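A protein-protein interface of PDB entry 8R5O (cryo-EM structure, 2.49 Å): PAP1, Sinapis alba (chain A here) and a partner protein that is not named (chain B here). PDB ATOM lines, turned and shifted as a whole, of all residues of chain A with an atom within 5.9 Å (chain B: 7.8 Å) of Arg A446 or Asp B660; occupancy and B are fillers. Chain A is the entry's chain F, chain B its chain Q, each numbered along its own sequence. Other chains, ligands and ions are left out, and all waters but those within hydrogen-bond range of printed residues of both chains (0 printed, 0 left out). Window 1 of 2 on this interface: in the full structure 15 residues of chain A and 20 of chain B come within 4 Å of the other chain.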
ATOM      1  N   TYR A 436      -4.282 -21.598  22.347  1.00  0.00           N
ATOM      2  CA  TYR A 436      -3.399 -21.358  21.211  1.00  0.00           C
ATOM      3  C   TYR A 436      -2.642 -20.044  21.361  1.00  0.00           C
ATOM      4  O   TYR A 436      -1.440 -19.977  21.083  1.00  0.00           O
ATOM      5  CB  TYR A 436      -4.214 -21.372  19.918  1.00  0.00           C
ATOM      6  CG  TYR A 436      -3.416 -21.109  18.666  1.00  0.00           C
ATOM      7  CD1 TYR A 436      -2.685 -22.120  18.061  1.00  0.00           C
ATOM      8  CD2 TYR A 436      -3.407 -19.854  18.078  1.00  0.00           C
ATOM      9  CE1 TYR A 436      -1.960 -21.885  16.915  1.00  0.00           C
ATOM     10  CE2 TYR A 436      -2.686 -19.610  16.932  1.00  0.00           C
ATOM     11  CZ  TYR A 436      -1.965 -20.630  16.354  1.00  0.00           C
ATOM     12  OH  TYR A 436      -1.243 -20.393  15.208  1.00  0.00           O
ATOM     13  N   GLU A 439      -0.040 -20.092  24.300  1.00  0.00           N
ATOM     14  CA  GLU A 439       1.088 -20.976  24.049  1.00  0.00           C
ATOM     15  C   GLU A 439       2.048 -20.416  23.008  1.00  0.00           C
ATOM     16  O   GLU A 439       2.940 -21.136  22.552  1.00  0.00           O
ATOM     17  CB  GLU A 439       0.594 -22.357  23.613  1.00  0.00           C
ATOM     18  CG  GLU A 439       0.017 -23.196  24.741  1.00  0.00           C
ATOM     19  CD  GLU A 439      -0.675 -24.450  24.240  1.00  0.00           C
ATOM     20  OE1 GLU A 439      -0.799 -24.610  23.009  1.00  0.00           O
ATOM     21  OE2 GLU A 439      -1.098 -25.273  25.079  1.00  0.00           O
ATOM     22  N   GLY A 440       1.886 -19.153  22.624  1.00  0.00           N
ATOM     23  CA  GLY A 440       2.760 -18.543  21.644  1.00  0.00           C
ATOM     24  C   GLY A 440       2.380 -18.778  20.202  1.00  0.00           C
ATOM     25  O   GLY A 440       3.249 -18.685  19.327  1.00  0.00           O
ATOM     26  N   GLY A 441       1.113 -19.076  19.919  1.00  0.00           N
ATOM     27  CA  GLY A 441       0.695 -19.375  18.562  1.00  0.00           C
ATOM     28  C   GLY A 441       0.616 -18.176  17.641  1.00  0.00           C
ATOM     29  O   GLY A 441       0.476 -18.362  16.428  1.00  0.00           O
ATOM     30  N   THR A 443       3.077 -15.814  17.400  1.00  0.00           N
ATOM     31  CA  THR A 443       4.406 -15.302  17.105  1.00  0.00           C
ATOM     32  C   THR A 443       5.377 -16.355  16.591  1.00  0.00           C
ATOM     33  O   THR A 443       6.562 -16.048  16.432  1.00  0.00           O
ATOM     34  CB  THR A 443       5.010 -14.636  18.352  1.00  0.00           C
ATOM     35  OG1 THR A 443       4.902 -15.524  19.470  1.00  0.00           O
ATOM     36  CG2 THR A 443       4.286 -13.336  18.669  1.00  0.00           C
ATOM     37  N   GLY A 444       4.921 -17.577  16.332  1.00  0.00           N
ATOM     38  CA  GLY A 444       5.814 -18.628  15.895  1.00  0.00           C
ATOM     39  C   GLY A 444       6.588 -19.305  17.001  1.00  0.00           C
ATOM     40  O   GLY A 444       7.498 -20.088  16.710  1.00  0.00           O
ATOM     41  N   GLU A 445       6.256 -19.029  18.261  1.00  0.00           N
ATOM     42  CA  GLU A 445       6.944 -19.601  19.407  1.00  0.00           C
ATOM     43  C   GLU A 445       6.188 -20.773  20.017  1.00  0.00           C
ATOM     44  O   GLU A 445       6.528 -21.211  21.121  1.00  0.00           O
ATOM     45  CB  GLU A 445       7.181 -18.521  20.466  1.00  0.00           C
ATOM     46  CG  GLU A 445       8.033 -17.361  19.980  1.00  0.00           C
ATOM     47  CD  GLU A 445       8.024 -16.189  20.940  1.00  0.00           C
ATOM     48  OE1 GLU A 445       7.053 -16.062  21.714  1.00  0.00           O
ATOM     49  OE2 GLU A 445       8.988 -15.394  20.922  1.00  0.00           O
ATOM     50  N   ARG A 446       5.174 -21.287  19.329  1.00  0.00           N
ATOM     51  CA  ARG A 446       4.375 -22.382  19.852  1.00  0.00           C
ATOM     52  C   ARG A 446       5.126 -23.704  19.742  1.00  0.00           C
ATOM     53  O   ARG A 446       5.952 -23.905  18.847  1.00  0.00           O
ATOM     54  CB  ARG A 446       3.042 -22.471  19.106  1.00  0.00           C
ATOM     55  CG  ARG A 446       2.067 -23.475  19.689  1.00  0.00           C
ATOM     56  CD  ARG A 446       0.799 -23.581  18.870  1.00  0.00           C
ATOM     57  NE  ARG A 446      -0.027 -24.694  19.320  1.00  0.00           N
ATOM     58  CZ  ARG A 446       0.023 -25.916  18.809  1.00  0.00           C
ATOM     59  NH1 ARG A 446       0.828 -26.213  17.804  1.00  0.00           N
ATOM     60  NH2 ARG A 446      -0.755 -26.865  19.322  1.00  0.00           N
ATOM     61  N   LYS A 447       4.830 -24.610  20.672  1.00  0.00           N
ATOM     62  CA  LYS A 447       5.395 -25.954  20.679  1.00  0.00           C
ATOM     63  C   LYS A 447       4.550 -26.844  19.773  1.00  0.00           C
ATOM     64  O   LYS A 447       3.389 -27.133  20.080  1.00  0.00           O
ATOM     65  CB  LYS A 447       5.450 -26.500  22.105  1.00  0.00           C
ATOM     66  CG  LYS A 447       5.577 -28.012  22.213  1.00  0.00           C
ATOM     67  CD  LYS A 447       6.912 -28.511  21.696  1.00  0.00           C
ATOM     68  CE  LYS A 447       7.013 -30.020  21.832  1.00  0.00           C
ATOM     69  NZ  LYS A 447       8.318 -30.536  21.342  1.00  0.00           N
ATOM     70  N   ARG A 448       5.130 -27.273  18.654  1.00  0.00           N
ATOM     71  CA  ARG A 448       4.442 -28.137  17.705  1.00  0.00           C
ATOM     72  C   ARG A 448       4.674 -29.596  18.074  1.00  0.00           C
ATOM     73  O   ARG A 448       5.817 -30.017  18.280  1.00  0.00           O
ATOM     74  CB  ARG A 448       4.929 -27.874  16.280  1.00  0.00           C
ATOM     75  CG  ARG A 448       4.124 -26.843  15.509  1.00  0.00           C
ATOM     76  CD  ARG A 448       4.288 -25.448  16.076  1.00  0.00           C
ATOM     77  NE  ARG A 448       3.688 -24.444  15.206  1.00  0.00           N
ATOM     78  CZ  ARG A 448       4.334 -23.816  14.235  1.00  0.00           C
ATOM     79  NH1 ARG A 448       5.613 -24.048  13.992  1.00  0.00           N
ATOM     80  NH2 ARG A 448       3.681 -22.931  13.487  1.00  0.00           N
ATOM     81  N   TRP A 449       3.592 -30.361  18.153  1.00  0.00           N
ATOM     82  CA  TRP A 449       3.670 -31.788  18.460  1.00  0.00           C
ATOM     83  C   TRP A 449       3.666 -32.615  17.176  1.00  0.00           C
ATOM     84  O   TRP A 449       2.816 -33.473  16.951  1.00  0.00           O
ATOM     85  CB  TRP A 449       2.528 -32.188  19.389  1.00  0.00           C
ATOM     86  CG  TRP A 449       2.627 -31.550  20.736  1.00  0.00           C
ATOM     87  CD1 TRP A 449       2.285 -30.273  21.063  1.00  0.00           C
ATOM     88  CD2 TRP A 449       3.110 -32.157  21.938  1.00  0.00           C
ATOM     89  NE1 TRP A 449       2.521 -30.046  22.395  1.00  0.00           N
ATOM     90  CE2 TRP A 449       3.029 -31.189  22.957  1.00  0.00           C
ATOM     91  CE3 TRP A 449       3.602 -33.427  22.253  1.00  0.00           C
ATOM     92  CZ2 TRP A 449       3.420 -31.449  24.267  1.00  0.00           C
ATOM     93  CZ3 TRP A 449       3.990 -33.684  23.555  1.00  0.00           C
ATOM     94  CH2 TRP A 449       3.896 -32.700  24.546  1.00  0.00           C
ATOM     95  N   VAL A 450       4.648 -32.337  16.330  1.00  0.00           N
ATOM     96  CA  VAL A 450       4.829 -33.008  15.047  1.00  0.00           C
ATOM     97  C   VAL A 450       6.030 -33.940  15.168  1.00  0.00           C
ATOM     98  O   VAL A 450       7.149 -33.465  15.402  1.00  0.00           O
ATOM     99  CB  VAL A 450       5.029 -32.002  13.904  1.00  0.00           C
ATOM    100  CG1 VAL A 450       5.287 -32.729  12.597  1.00  0.00           C
ATOM    101  CG2 VAL A 450       3.821 -31.091  13.785  1.00  0.00           C
ATOM    102  N   ARG B 626      -1.291 -16.219  11.469  1.00  0.00           N
ATOM    103  CA  ARG B 626      -1.152 -17.351  12.375  1.00  0.00           C
ATOM    104  C   ARG B 626      -2.315 -17.480  13.348  1.00  0.00           C
ATOM    105  O   ARG B 626      -2.441 -18.524  13.995  1.00  0.00           O
ATOM    106  CB  ARG B 626       0.160 -17.238  13.155  1.00  0.00           C
ATOM    107  CG  ARG B 626       1.344 -16.808  12.309  1.00  0.00           C
ATOM    108  CD  ARG B 626       2.640 -16.849  13.101  1.00  0.00           C
ATOM    109  NE  ARG B 626       3.252 -18.171  13.080  1.00  0.00           N
ATOM    110  CZ  ARG B 626       4.218 -18.535  12.249  1.00  0.00           C
ATOM    111  NH1 ARG B 626       4.719 -17.693  11.361  1.00  0.00           N
ATOM    112  NH2 ARG B 626       4.696 -19.774  12.312  1.00  0.00           N
ATOM    113  N   ARG B 629      -5.562 -20.032  12.163  1.00  0.00           N
ATOM    114  CA  ARG B 629      -5.374 -21.466  11.945  1.00  0.00           C
ATOM    115  C   ARG B 629      -6.236 -22.324  12.862  1.00  0.00           C
ATOM    116  O   ARG B 629      -6.921 -23.229  12.354  1.00  0.00           O
ATOM    117  CB  ARG B 629      -3.886 -21.811  12.072  1.00  0.00           C
ATOM    118  CG  ARG B 629      -3.007 -21.052  11.102  1.00  0.00           C
ATOM    119  CD  ARG B 629      -1.543 -21.337  11.342  1.00  0.00           C
ATOM    120  NE  ARG B 629      -0.701 -20.649  10.373  1.00  0.00           N
ATOM    121  CZ  ARG B 629       0.623 -20.682  10.374  1.00  0.00           C
ATOM    122  NH1 ARG B 629       1.296 -21.365  11.284  1.00  0.00           N
ATOM    123  NH2 ARG B 629       1.290 -20.014   9.438  1.00  0.00           N
ATOM    124  N   PRO B 630      -6.264 -22.120  14.184  1.00  0.00           N
ATOM    125  CA  PRO B 630      -7.210 -22.895  14.998  1.00  0.00           C
ATOM    126  C   PRO B 630      -8.652 -22.476  14.795  1.00  0.00           C
ATOM    127  O   PRO B 630      -9.558 -23.292  15.006  1.00  0.00           O
ATOM    128  CB  PRO B 630      -6.739 -22.623  16.432  1.00  0.00           C
ATOM    129  CG  PRO B 630      -6.115 -21.299  16.359  1.00  0.00           C
ATOM    130  CD  PRO B 630      -5.437 -21.235  15.025  1.00  0.00           C
ATOM    131  N   THR B 633     -10.380 -24.212  11.667  1.00  0.00           N
ATOM    132  CA  THR B 633     -10.609 -25.638  11.868  1.00  0.00           C
ATOM    133  C   THR B 633     -11.830 -25.879  12.745  1.00  0.00           C
ATOM    134  O   THR B 633     -12.612 -26.802  12.491  1.00  0.00           O
ATOM    135  CB  THR B 633      -9.371 -26.286  12.483  1.00  0.00           C
ATOM    136  OG1 THR B 633      -8.246 -26.056  11.629  1.00  0.00           O
ATOM    137  CG2 THR B 633      -9.576 -27.781  12.649  1.00  0.00           C
ATOM    138  N   LEU B 645      -8.235 -31.210   5.994  1.00  0.00           N
ATOM    139  CA  LEU B 645      -7.202 -30.196   6.127  1.00  0.00           C
ATOM    140  C   LEU B 645      -6.068 -30.470   5.151  1.00  0.00           C
ATOM    141  O   LEU B 645      -5.737 -31.621   4.859  1.00  0.00           O
ATOM    142  CB  LEU B 645      -6.664 -30.158   7.557  1.00  0.00           C
ATOM    143  CG  LEU B 645      -7.703 -30.008   8.668  1.00  0.00           C
ATOM    144  CD1 LEU B 645      -7.026 -29.908  10.024  1.00  0.00           C
ATOM    145  CD2 LEU B 645      -8.588 -28.800   8.415  1.00  0.00           C
ATOM    146  N   ASP B 654       7.021 -25.296   7.261  1.00  0.00           N
ATOM    147  CA  ASP B 654       6.730 -26.704   7.023  1.00  0.00           C
ATOM    148  C   ASP B 654       5.223 -26.934   7.047  1.00  0.00           C
ATOM    149  O   ASP B 654       4.546 -26.471   7.974  1.00  0.00           O
ATOM    150  CB  ASP B 654       7.422 -27.572   8.070  1.00  0.00           C
ATOM    151  CG  ASP B 654       7.217 -29.054   7.829  1.00  0.00           C
ATOM    152  OD1 ASP B 654       7.717 -29.567   6.806  1.00  0.00           O
ATOM    153  OD2 ASP B 654       6.558 -29.707   8.664  1.00  0.00           O
ATOM    154  N   PRO B 655       4.660 -27.625   6.052  1.00  0.00           N
ATOM    155  CA  PRO B 655       3.199 -27.805   6.018  1.00  0.00           C
ATOM    156  C   PRO B 655       2.639 -28.547   7.217  1.00  0.00           C
ATOM    157  O   PRO B 655       1.502 -28.274   7.622  1.00  0.00           O
ATOM    158  CB  PRO B 655       2.976 -28.584   4.713  1.00  0.00           C
ATOM    159  CG  PRO B 655       4.285 -29.224   4.418  1.00  0.00           C
ATOM    160  CD  PRO B 655       5.325 -28.269   4.909  1.00  0.00           C
ATOM    161  N   LEU B 656       3.392 -29.480   7.803  1.00  0.00           N
ATOM    162  CA  LEU B 656       2.886 -30.210   8.959  1.00  0.00           C
ATOM    163  C   LEU B 656       2.867 -29.359  10.221  1.00  0.00           C
ATOM    164  O   LEU B 656       2.144 -29.691  11.165  1.00  0.00           O
ATOM    165  CB  LEU B 656       3.715 -31.475   9.191  1.00  0.00           C
ATOM    166  CG  LEU B 656       3.620 -32.552   8.108  1.00  0.00           C
ATOM    167  CD1 LEU B 656       4.361 -33.807   8.535  1.00  0.00           C
ATOM    168  CD2 LEU B 656       2.169 -32.866   7.789  1.00  0.00           C
ATOM    169  N   ASP B 657       3.648 -28.277  10.263  1.00  0.00           N
ATOM    170  CA  ASP B 657       3.590 -27.362  11.396  1.00  0.00           C
ATOM    171  C   ASP B 657       2.339 -26.495  11.346  1.00  0.00           C
ATOM    172  O   ASP B 657       1.728 -26.221  12.385  1.00  0.00           O
ATOM    173  CB  ASP B 657       4.842 -26.487  11.435  1.00  0.00           C
ATOM    174  CG  ASP B 657       6.077 -27.257  11.850  1.00  0.00           C
ATOM    175  OD1 ASP B 657       6.498 -28.160  11.098  1.00  0.00           O
ATOM    176  OD2 ASP B 657       6.630 -26.961  12.930  1.00  0.00           O
ATOM    177  N   ILE B 658       1.948 -26.055  10.150  1.00  0.00           N
ATOM    178  CA  ILE B 658       0.706 -25.305  10.000  1.00  0.00           C
ATOM    179  C   ILE B 658      -0.488 -26.182  10.351  1.00  0.00           C
ATOM    180  O   ILE B 658      -1.415 -25.747  11.043  1.00  0.00           O
ATOM    181  CB  ILE B 658       0.592 -24.743   8.571  1.00  0.00           C
ATOM    182  CG1 ILE B 658       1.868 -23.995   8.195  1.00  0.00           C
ATOM    183  CG2 ILE B 658      -0.619 -23.833   8.452  1.00  0.00           C
ATOM    184  CD1 ILE B 658       1.912 -23.567   6.756  1.00  0.00           C
ATOM    185  N   LEU B 659      -0.483 -27.431   9.879  1.00  0.00           N
ATOM    186  CA  LEU B 659      -1.579 -28.344  10.183  1.00  0.00           C
ATOM    187  C   LEU B 659      -1.652 -28.659  11.670  1.00  0.00           C
ATOM    188  O   LEU B 659      -2.739 -28.922  12.195  1.00  0.00           O
ATOM    189  CB  LEU B 659      -1.431 -29.630   9.373  1.00  0.00           C
ATOM    190  CG  LEU B 659      -1.643 -29.505   7.864  1.00  0.00           C
ATOM    191  CD1 LEU B 659      -1.305 -30.806   7.155  1.00  0.00           C
ATOM    192  CD2 LEU B 659      -3.073 -29.096   7.573  1.00  0.00           C
ATOM    193  N   ASP B 660      -0.512 -28.647  12.364  1.00  0.00           N
ATOM    194  CA  ASP B 660      -0.531 -28.821  13.812  1.00  0.00           C
ATOM    195  C   ASP B 660      -1.215 -27.644  14.496  1.00  0.00           C
ATOM    196  O   ASP B 660      -1.961 -27.829  15.464  1.00  0.00           O
ATOM    197  CB  ASP B 660       0.891 -28.999  14.340  1.00  0.00           C
ATOM    198  CG  ASP B 660       0.930 -29.253  15.833  1.00  0.00           C
ATOM    199  OD1 ASP B 660       0.521 -30.351  16.260  1.00  0.00           O
ATOM    200  OD2 ASP B 660       1.366 -28.351  16.579  1.00  0.00           O
ATOM    201  N   ASP B 661      -0.966 -26.424  14.011  1.00  0.00           N
ATOM    202  CA  ASP B 661      -1.659 -25.258  14.549  1.00  0.00           C
ATOM    203  C   ASP B 661      -3.155 -25.336  14.279  1.00  0.00           C
ATOM    204  O   ASP B 661      -3.968 -24.977  15.138  1.00  0.00           O
ATOM    205  CB  ASP B 661      -1.074 -23.977  13.955  1.00  0.00           C
ATOM    206  CG  ASP B 661       0.332 -23.700  14.436  1.00  0.00           C
ATOM    207  OD1 ASP B 661       0.664 -24.107  15.568  1.00  0.00           O
ATOM    208  OD2 ASP B 661       1.106 -23.073  13.686  1.00  0.00           O
ATOM    209  N   MET B 662      -3.536 -25.793  13.086  1.00  0.00           N
ATOM    210  CA  MET B 662      -4.952 -25.962  12.774  1.00  0.00           C
ATOM    211  C   MET B 662      -5.590 -27.022  13.661  1.00  0.00           C
ATOM    212  O   MET B 662      -6.707 -26.837  14.156  1.00  0.00           O
ATOM    213  CB  MET B 662      -5.123 -26.318  11.297  1.00  0.00           C
ATOM    214  CG  MET B 662      -4.569 -25.276  10.341  1.00  0.00           C
ATOM    215  SD  MET B 662      -4.816 -25.702   8.608  1.00  0.00           S
ATOM    216  CE  MET B 662      -6.602 -25.658   8.498  1.00  0.00           C
ATOM    217  N   LEU B 663      -4.893 -28.141  13.878  1.00  0.00           N
ATOM    218  CA  LEU B 663      -5.441 -29.217  14.698  1.00  0.00           C
ATOM    219  C   LEU B 663      -5.665 -28.778  16.139  1.00  0.00           C
ATOM    220  O   LEU B 663      -6.539 -29.322  16.823  1.00  0.00           O
ATOM    221  CB  LEU B 663      -4.517 -30.435  14.657  1.00  0.00           C
ATOM    222  CG  LEU B 663      -4.578 -31.312  13.409  1.00  0.00           C
ATOM    223  CD1 LEU B 663      -3.510 -32.390  13.463  1.00  0.00           C
ATOM    224  CD2 LEU B 663      -5.957 -31.931  13.269  1.00  0.00           C
ATOM    225  N   SER B 664      -4.890 -27.804  16.617  1.00  0.00           N
ATOM    226  CA  SER B 664      -5.019 -27.354  17.998  1.00  0.00           C
ATOM    227  C   SER B 664      -6.364 -26.696  18.275  1.00  0.00           C
ATOM    228  O   SER B 664      -6.754 -26.578  19.442  1.00  0.00           O
ATOM    229  CB  SER B 664      -3.891 -26.384  18.339  1.00  0.00           C
ATOM    230  OG  SER B 664      -3.929 -25.247  17.496  1.00  0.00           O
ATOM    231  N   GLY B 665      -7.081 -26.266  17.238  1.00  0.00           N
ATOM    232  CA  GLY B 665      -8.368 -25.626  17.437  1.00  0.00           C
ATOM    233  C   GLY B 665      -9.482 -26.565  17.838  1.00  0.00           C
ATOM    234  O   GLY B 665     -10.538 -26.092  18.273  1.00  0.00           O
ATOM    235  N   ILE B 666      -9.280 -27.874  17.701  1.00  0.00           N
ATOM    236  CA  ILE B 666     -10.252 -28.872  18.116  1.00  0.00           C
ATOM    237  C   ILE B 666      -9.693 -29.802  19.185  1.00  0.00           C
ATOM    238  O   ILE B 666     -10.356 -30.763  19.574  1.00  0.00           O
ATOM    239  CB  ILE B 666     -10.776 -29.679  16.911  1.00  0.00           C
ATOM    240  CG1 ILE B 666      -9.629 -30.420  16.225  1.00  0.00           C
ATOM    241  CG2 ILE B 666     -11.487 -28.765  15.930  1.00  0.00           C
ATOM    242  CD1 ILE B 666     -10.075 -31.311  15.094  1.00  0.00           C
ATOM    243  N   TRP B 668      -6.612 -31.505  18.999  1.00  0.00           N
ATOM    244  CA  TRP B 668      -5.794 -32.579  18.458  1.00  0.00           C
ATOM    245  C   TRP B 668      -4.368 -32.101  18.223  1.00  0.00           C
ATOM    246  O   TRP B 668      -4.055 -30.912  18.307  1.00  0.00           O
ATOM    247  CB  TRP B 668      -6.384 -33.114  17.148  1.00  0.00           C
ATOM    248  CG  TRP B 668      -7.618 -33.937  17.315  1.00  0.00           C
ATOM    249  CD1 TRP B 668      -8.567 -33.807  18.283  1.00  0.00           C
ATOM    250  CD2 TRP B 668      -8.032 -35.032  16.492  1.00  0.00           C
ATOM    251  NE1 TRP B 668      -9.551 -34.747  18.111  1.00  0.00           N
ATOM    252  CE2 TRP B 668      -9.246 -35.513  17.016  1.00  0.00           C
ATOM    253  CE3 TRP B 668      -7.495 -35.650  15.358  1.00  0.00           C
ATOM    254  CZ2 TRP B 668      -9.933 -36.583  16.449  1.00  0.00           C
ATOM    255  CZ3 TRP B 668      -8.178 -36.712  14.795  1.00  0.00           C
ATOM    256  CH2 TRP B 668      -9.383 -37.168  15.341  1.00  0.00           C
ATOM    257  N   THR B 669      -3.500 -33.063  17.923  1.00  0.00           N
ATOM    258  CA  THR B 669      -2.131 -32.791  17.517  1.00  0.00           C
ATOM    259  C   THR B 669      -1.771 -33.723  16.372  1.00  0.00           C
ATOM    260  O   THR B 669      -2.422 -34.746  16.151  1.00  0.00           O
ATOM    261  CB  THR B 669      -1.135 -32.959  18.673  1.00  0.00           C
ATOM    262  OG1 THR B 669      -1.485 -34.111  19.449  1.00  0.00           O
ATOM    263  CG2 THR B 669      -1.133 -31.724  19.557  1.00  0.00           C
ATOM    264  N   MET B 670      -0.726 -33.349  15.633  1.00  0.00           N
ATOM    265  CA  MET B 670      -0.296 -34.166  14.505  1.00  0.00           C
ATOM    266  C   MET B 670       0.130 -35.554  14.962  1.00  0.00           C
ATOM    267  O   MET B 670      -0.126 -36.548  14.274  1.00  0.00           O
ATOM    268  CB  MET B 670       0.841 -33.473  13.756  1.00  0.00           C
ATOM    269  CG  MET B 670       1.345 -34.246  12.552  1.00  0.00           C
ATOM    270  SD  MET B 670       0.065 -34.526  11.313  1.00  0.00           S
ATOM    271  CE  MET B 670      -0.268 -32.849  10.789  1.00  0.00           C
ATOM    272  N   GLN B 671       0.775 -35.641  16.127  1.00  0.00           N
ATOM    273  CA  GLN B 671       1.210 -36.934  16.642  1.00  0.00           C
ATOM    274  C   GLN B 671       0.027 -37.853  16.914  1.00  0.00           C
ATOM    275  O   GLN B 671       0.069 -39.045  16.587  1.00  0.00           O
ATOM    276  CB  GLN B 671       2.038 -36.736  17.911  1.00  0.00           C
ATOM    277  CG  GLN B 671       2.551 -38.024  18.522  1.00  0.00           C
ATOM    278  CD  GLN B 671       3.300 -37.796  19.814  1.00  0.00           C
ATOM    279  OE1 GLN B 671       4.514 -37.989  19.883  1.00  0.00           O
ATOM    280  NE2 GLN B 671       2.580 -37.386  20.850  1.00  0.00           N
ATOM    281  N   GLU B 672      -1.039 -37.320  17.517  1.00  0.00           N
ATOM    282  CA  GLU B 672      -2.219 -38.135  17.787  1.00  0.00           C
ATOM    283  C   GLU B 672      -2.892 -38.582  16.495  1.00  0.00           C
ATOM    284  O   GLU B 672      -3.360 -39.722  16.392  1.00  0.00           O
ATOM    285  CB  GLU B 672      -3.204 -37.366  18.666  1.00  0.00           C
ATOM    286  CG  GLU B 672      -2.689 -37.081  20.065  1.00  0.00           C
ATOM    287  CD  GLU B 672      -3.722 -36.398  20.936  1.00  0.00           C
ATOM    288  OE1 GLU B 672      -4.839 -36.135  20.441  1.00  0.00           O
ATOM    289  OE2 GLU B 672      -3.418 -36.124  22.116  1.00  0.00           O
ATOM    290  N   LEU B 693      -6.785 -35.569   6.945  1.00  0.00           N
ATOM    291  CA  LEU B 693      -5.638 -34.684   6.825  1.00  0.00           C
ATOM    292  C   LEU B 693      -4.669 -35.230   5.788  1.00  0.00           C
ATOM    293  O   LEU B 693      -4.465 -36.443   5.698  1.00  0.00           O
ATOM    294  CB  LEU B 693      -4.952 -34.526   8.189  1.00  0.00           C
ATOM    295  CG  LEU B 693      -3.791 -33.554   8.376  1.00  0.00           C
ATOM    296  CD1 LEU B 693      -3.837 -32.990   9.779  1.00  0.00           C
ATOM    297  CD2 LEU B 693      -2.467 -34.249   8.136  1.00  0.00           C
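Asp B660 touches just these residues of chain A: Arg A446, Arg A448, Trp A449 and Val A450. Of the printed residues of chain B, Trp A449 touches Asp B660, Thr B669, Met B670 and Gln B671. Printed residues of chain B within 4 Å of Val A450: Leu B656 (3.4 Å), Asp B660 (3.6 Å) and Met B670 (3.8 Å). Of the printed residues of chain A, Ser B664 touches Tyr A436 (3.4 Å) and Arg A446 (3.3 Å). Met B662 touches none of the printed residues of chain A. The nearest residue of chain B that does not touch Arg A446 is Thr B669 (4.9 Å). The nearest printed residue of chain A that does not touch Asp B657 is Val A450 (4.4 Å).
Printed residues of chain B that touch a printed residue of chain A: Arg B626, Arg B629, Pro B630, Leu B656, Asp B657, Asp B660, Asp B661, Ser B664, Thr B669, Met B670 and Gln B671. Hydrophobic or aromatic side chains of chain A that line the printed part of chain B: Tyr A436, Trp A449 and Val A450. Among the printed residues, Asp or Glu carboxylates within 4 Å of a Lys or Arg side-chain nitrogen of the other chain: Arg A446 with Asp B660 (2.5 Å), Arg A446 with Asp B661 (3.1 Å), Arg A448 with Asp B657 (3.3 Å) and Arg A448 with Asp B661 (2.6 Å).
The side-chain carboxylate of Asp B660 lies within hydrogen-bond range of the backbone NH of Trp A449 (3.4 Å). OH of Tyr A436 is in hydrogen-bond range of O of Arg B626, 2.5 Å away. The guanidinium group of Arg A448 is in salt-bridge range of the side-chain carboxylate of Asp B657 (3.3 Å). OD2 of Asp B660 is in salt-bridge range of NH1 of Arg A446 (2.5 Å). The side-chain carboxylate (OD1) of Asp B661 lies within salt-bridge range of the guanidinium group (NH1) of Arg A446 (3.1 Å). The side-chain carboxylate (OD2) of Asp B661 lies within salt-bridge range of the guanidinium group (NH2) of Arg A448. N of Gln B671 sits at hydrogen-bond distance from O of Trp A449 (3.1 Å).
The side-chain carboxylate of Glu A439 lies within salt-bridge range of the guanidinium group of Arg A446 (3.8 Å). OD1 of Asp B660 sits at hydrogen-bond distance from N of Met B670, 3.3 Å away. OD2 of Asp B654 lies close to N of Leu B656 (3.3 Å). The side-chain hydroxyl (OH) of Tyr A436 lies within hydrogen-bond range of the backbone carbonyl oxygen (O) of Gly A441, 2.9 Å away. The backbone carbonyl oxygen (O) of Arg B629 sits at hydrogen-bond distance from the side-chain hydroxyl (OG1) of Thr B633 (3.2 Å). OD2 of Asp B661 lies within salt-bridge range of NH1 of Arg B629.
Tyr A436 touches Arg B629. Tyr A436 touches Pro B630 (CD2 to CG, 3.5 Å). Gly A441 touches Arg B626. Arg A446 touches Ser B664. NH2 of Arg A448 touches NH2 of Arg B626, 3.5 Å away. Asp B660 touches Arg A448 (OD2 to CA, 3.3 Å). Trp A449 touches Thr B669. CB of Met B670 touches O of Trp A449, at 3.8 Å. Leu B656 touches Val A450 (O to CG2, 3.4 Å). CG2 of Val A450 touches CB of Asp B660, 3.6 Å away.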
